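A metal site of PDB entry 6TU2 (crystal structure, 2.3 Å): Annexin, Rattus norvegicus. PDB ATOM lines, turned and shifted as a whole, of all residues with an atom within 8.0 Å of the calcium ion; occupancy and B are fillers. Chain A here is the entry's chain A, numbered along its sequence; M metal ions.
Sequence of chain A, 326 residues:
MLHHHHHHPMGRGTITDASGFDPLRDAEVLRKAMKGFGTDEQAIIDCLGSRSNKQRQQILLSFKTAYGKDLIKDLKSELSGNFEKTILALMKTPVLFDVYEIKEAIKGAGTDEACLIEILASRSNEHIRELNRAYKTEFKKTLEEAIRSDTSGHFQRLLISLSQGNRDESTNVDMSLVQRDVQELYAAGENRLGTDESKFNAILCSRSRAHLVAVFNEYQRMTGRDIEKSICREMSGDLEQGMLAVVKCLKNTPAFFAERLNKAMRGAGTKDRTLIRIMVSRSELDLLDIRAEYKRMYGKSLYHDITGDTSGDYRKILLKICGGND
The side-chain carboxylate (OE2) of Glu 240 lies within hydrogen-bond range of the side-chain amide nitrogen (NE2) of Gln 241, at 3.3 Å.
Three residues have an atom within 4 Å of the calcium ion: Cys 232, Met 235 and Glu 240. The nearest printed residue that does not touch the calcium ion is Ser 236 (4.04 Å).
The calcium ion is bound by O of Cys 232, O of Met 235 and OE1 of Glu 240.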
ATOM      1  N   LYS A 229       6.062 -24.957  23.161  1.00  0.00           N
ATOM      2  CA  LYS A 229       5.207 -25.305  24.290  1.00  0.00           C
ATOM      3  C   LYS A 229       5.793 -26.473  25.080  1.00  0.00           C
ATOM      4  O   LYS A 229       5.741 -26.470  26.322  1.00  0.00           O
ATOM      5  CB  LYS A 229       3.800 -25.636  23.802  1.00  0.00           C
ATOM      6  CG  LYS A 229       3.030 -24.421  23.295  1.00  0.00           C
ATOM      7  CD  LYS A 229       2.581 -23.526  24.446  1.00  0.00           C
ATOM      8  CE  LYS A 229       1.798 -22.315  23.943  1.00  0.00           C
ATOM      9  NZ  LYS A 229       2.626 -21.434  23.071  1.00  0.00           N
ATOM     10  N   SER A 230       6.351 -27.468  24.392  1.00  0.00           N
ATOM     11  CA  SER A 230       7.045 -28.542  25.103  1.00  0.00           C
ATOM     12  C   SER A 230       8.169 -27.979  25.967  1.00  0.00           C
ATOM     13  O   SER A 230       8.356 -28.414  27.113  1.00  0.00           O
ATOM     14  CB  SER A 230       7.603 -29.563  24.105  1.00  0.00           C
ATOM     15  OG  SER A 230       6.560 -30.276  23.459  1.00  0.00           O
ATOM     16  N   ILE A 231       8.910 -27.006  25.441  1.00  0.00           N
ATOM     17  CA  ILE A 231       9.989 -26.382  26.216  1.00  0.00           C
ATOM     18  C   ILE A 231       9.416 -25.700  27.456  1.00  0.00           C
ATOM     19  O   ILE A 231       9.941 -25.867  28.567  1.00  0.00           O
ATOM     20  CB  ILE A 231      10.767 -25.393  25.319  1.00  0.00           C
ATOM     21  CG1 ILE A 231      11.685 -26.164  24.370  1.00  0.00           C
ATOM     22  CG2 ILE A 231      11.562 -24.417  26.180  1.00  0.00           C
ATOM     23  CD1 ILE A 231      12.059 -25.390  23.132  1.00  0.00           C
ATOM     24  N   CYS A 232       8.352 -24.925  27.279  1.00  0.00           N
ATOM     25  CA  CYS A 232       7.721 -24.271  28.423  1.00  0.00           C
ATOM     26  C   CYS A 232       7.172 -25.292  29.412  1.00  0.00           C
ATOM     27  O   CYS A 232       7.193 -25.054  30.624  1.00  0.00           O
ATOM     28  CB  CYS A 232       6.605 -23.340  27.957  1.00  0.00           C
ATOM     29  SG  CYS A 232       7.190 -21.865  27.124  1.00  0.00           S
ATOM     30  N   ARG A 233       6.685 -26.426  28.920  1.00  0.00           N
ATOM     31  CA  ARG A 233       6.164 -27.459  29.811  1.00  0.00           C
ATOM     32  C   ARG A 233       7.283 -28.172  30.540  1.00  0.00           C
ATOM     33  O   ARG A 233       7.164 -28.489  31.738  1.00  0.00           O
ATOM     34  CB  ARG A 233       5.312 -28.452  29.020  1.00  0.00           C
ATOM     35  CG  ARG A 233       3.806 -28.297  29.196  1.00  0.00           C
ATOM     36  CD  ARG A 233       3.035 -29.002  28.076  1.00  0.00           C
ATOM     37  NE  ARG A 233       2.470 -28.048  27.133  1.00  0.00           N
ATOM     38  CZ  ARG A 233       1.168 -27.894  26.884  1.00  0.00           C
ATOM     39  NH1 ARG A 233       0.260 -28.656  27.482  1.00  0.00           N
ATOM     40  NH2 ARG A 233       0.766 -26.985  26.000  1.00  0.00           N
ATOM     41  N   GLU A 234       8.400 -28.434  29.856  1.00  0.00           N
ATOM     42  CA  GLU A 234       9.463 -29.247  30.421  1.00  0.00           C
ATOM     43  C   GLU A 234      10.458 -28.445  31.258  1.00  0.00           C
ATOM     44  O   GLU A 234      11.029 -28.994  32.207  1.00  0.00           O
ATOM     45  CB  GLU A 234      10.234 -29.960  29.302  1.00  0.00           C
ATOM     46  CG  GLU A 234       9.423 -31.015  28.559  1.00  0.00           C
ATOM     47  CD  GLU A 234       8.931 -32.109  29.479  1.00  0.00           C
ATOM     48  OE1 GLU A 234       7.740 -32.488  29.354  1.00  0.00           O
ATOM     49  OE2 GLU A 234       9.712 -32.582  30.332  1.00  0.00           O
ATOM     50  N   MET A 235      10.689 -27.185  30.924  1.00  0.00           N
ATOM     51  CA  MET A 235      11.750 -26.410  31.542  1.00  0.00           C
ATOM     52  C   MET A 235      11.200 -25.151  32.196  1.00  0.00           C
ATOM     53  O   MET A 235      10.117 -24.667  31.861  1.00  0.00           O
ATOM     54  CB  MET A 235      12.818 -26.038  30.506  1.00  0.00           C
ATOM     55  CG  MET A 235      13.651 -27.229  30.067  1.00  0.00           C
ATOM     56  SD  MET A 235      14.355 -27.025  28.417  1.00  0.00           S
ATOM     57  CE  MET A 235      14.837 -28.717  28.060  1.00  0.00           C
ATOM     58  N   SER A 236      11.970 -24.634  33.141  1.00  0.00           N
ATOM     59  CA  SER A 236      11.648 -23.406  33.856  1.00  0.00           C
ATOM     60  C   SER A 236      12.917 -22.602  34.041  1.00  0.00           C
ATOM     61  O   SER A 236      14.032 -23.089  33.811  1.00  0.00           O
ATOM     62  CB  SER A 236      11.000 -23.705  35.211  1.00  0.00           C
ATOM     63  OG  SER A 236      11.891 -24.423  36.045  1.00  0.00           O
ATOM     64  N   GLY A 237      12.747 -21.350  34.464  1.00  0.00           N
ATOM     65  CA  GLY A 237      13.895 -20.518  34.763  1.00  0.00           C
ATOM     66  C   GLY A 237      14.683 -20.144  33.517  1.00  0.00           C
ATOM     67  O   GLY A 237      14.202 -20.216  32.379  1.00  0.00           O
ATOM     68  N   GLU A 240      14.790 -22.246  30.459  1.00  0.00           N
ATOM     69  CA  GLU A 240      13.623 -22.125  29.598  1.00  0.00           C
ATOM     70  C   GLU A 240      13.757 -20.934  28.662  1.00  0.00           C
ATOM     71  O   GLU A 240      13.609 -21.067  27.443  1.00  0.00           O
ATOM     72  CB  GLU A 240      12.356 -22.013  30.447  1.00  0.00           C
ATOM     73  CG  GLU A 240      11.069 -22.048  29.640  1.00  0.00           C
ATOM     74  CD  GLU A 240       9.911 -21.392  30.366  1.00  0.00           C
ATOM     75  OE1 GLU A 240       9.345 -22.018  31.296  1.00  0.00           O
ATOM     76  OE2 GLU A 240       9.563 -20.244  30.011  1.00  0.00           O
ATOM     77  N   GLN A 241      14.029 -19.751  29.233  1.00  0.00           N
ATOM     78  CA  GLN A 241      14.203 -18.568  28.395  1.00  0.00           C
ATOM     79  C   GLN A 241      15.321 -18.761  27.378  1.00  0.00           C
ATOM     80  O   GLN A 241      15.233 -18.249  26.254  1.00  0.00           O
ATOM     81  CB  GLN A 241      14.497 -17.337  29.265  1.00  0.00           C
ATOM     82  CG  GLN A 241      13.391 -16.980  30.240  1.00  0.00           C
ATOM     83  CD  GLN A 241      12.069 -16.668  29.547  1.00  0.00           C
ATOM     84  OE1 GLN A 241      12.010 -15.854  28.629  1.00  0.00           O
ATOM     85  NE2 GLN A 241      11.003 -17.314  29.995  1.00  0.00           N
ATOM     86  N   LEU A 244      13.986 -21.142  24.438  1.00  0.00           N
ATOM     87  CA  LEU A 244      13.026 -20.409  23.616  1.00  0.00           C
ATOM     88  C   LEU A 244      13.735 -19.364  22.753  1.00  0.00           C
ATOM     89  O   LEU A 244      13.459 -19.245  21.545  1.00  0.00           O
ATOM     90  CB  LEU A 244      11.973 -19.757  24.508  1.00  0.00           C
ATOM     91  CG  LEU A 244      10.992 -20.718  25.170  1.00  0.00           C
ATOM     92  CD1 LEU A 244      10.179 -20.011  26.248  1.00  0.00           C
ATOM     93  CD2 LEU A 244      10.077 -21.347  24.138  1.00  0.00           C
HETATM   94 CA    CA M   1       7.871 -24.114  32.625  1.00  0.00          CA
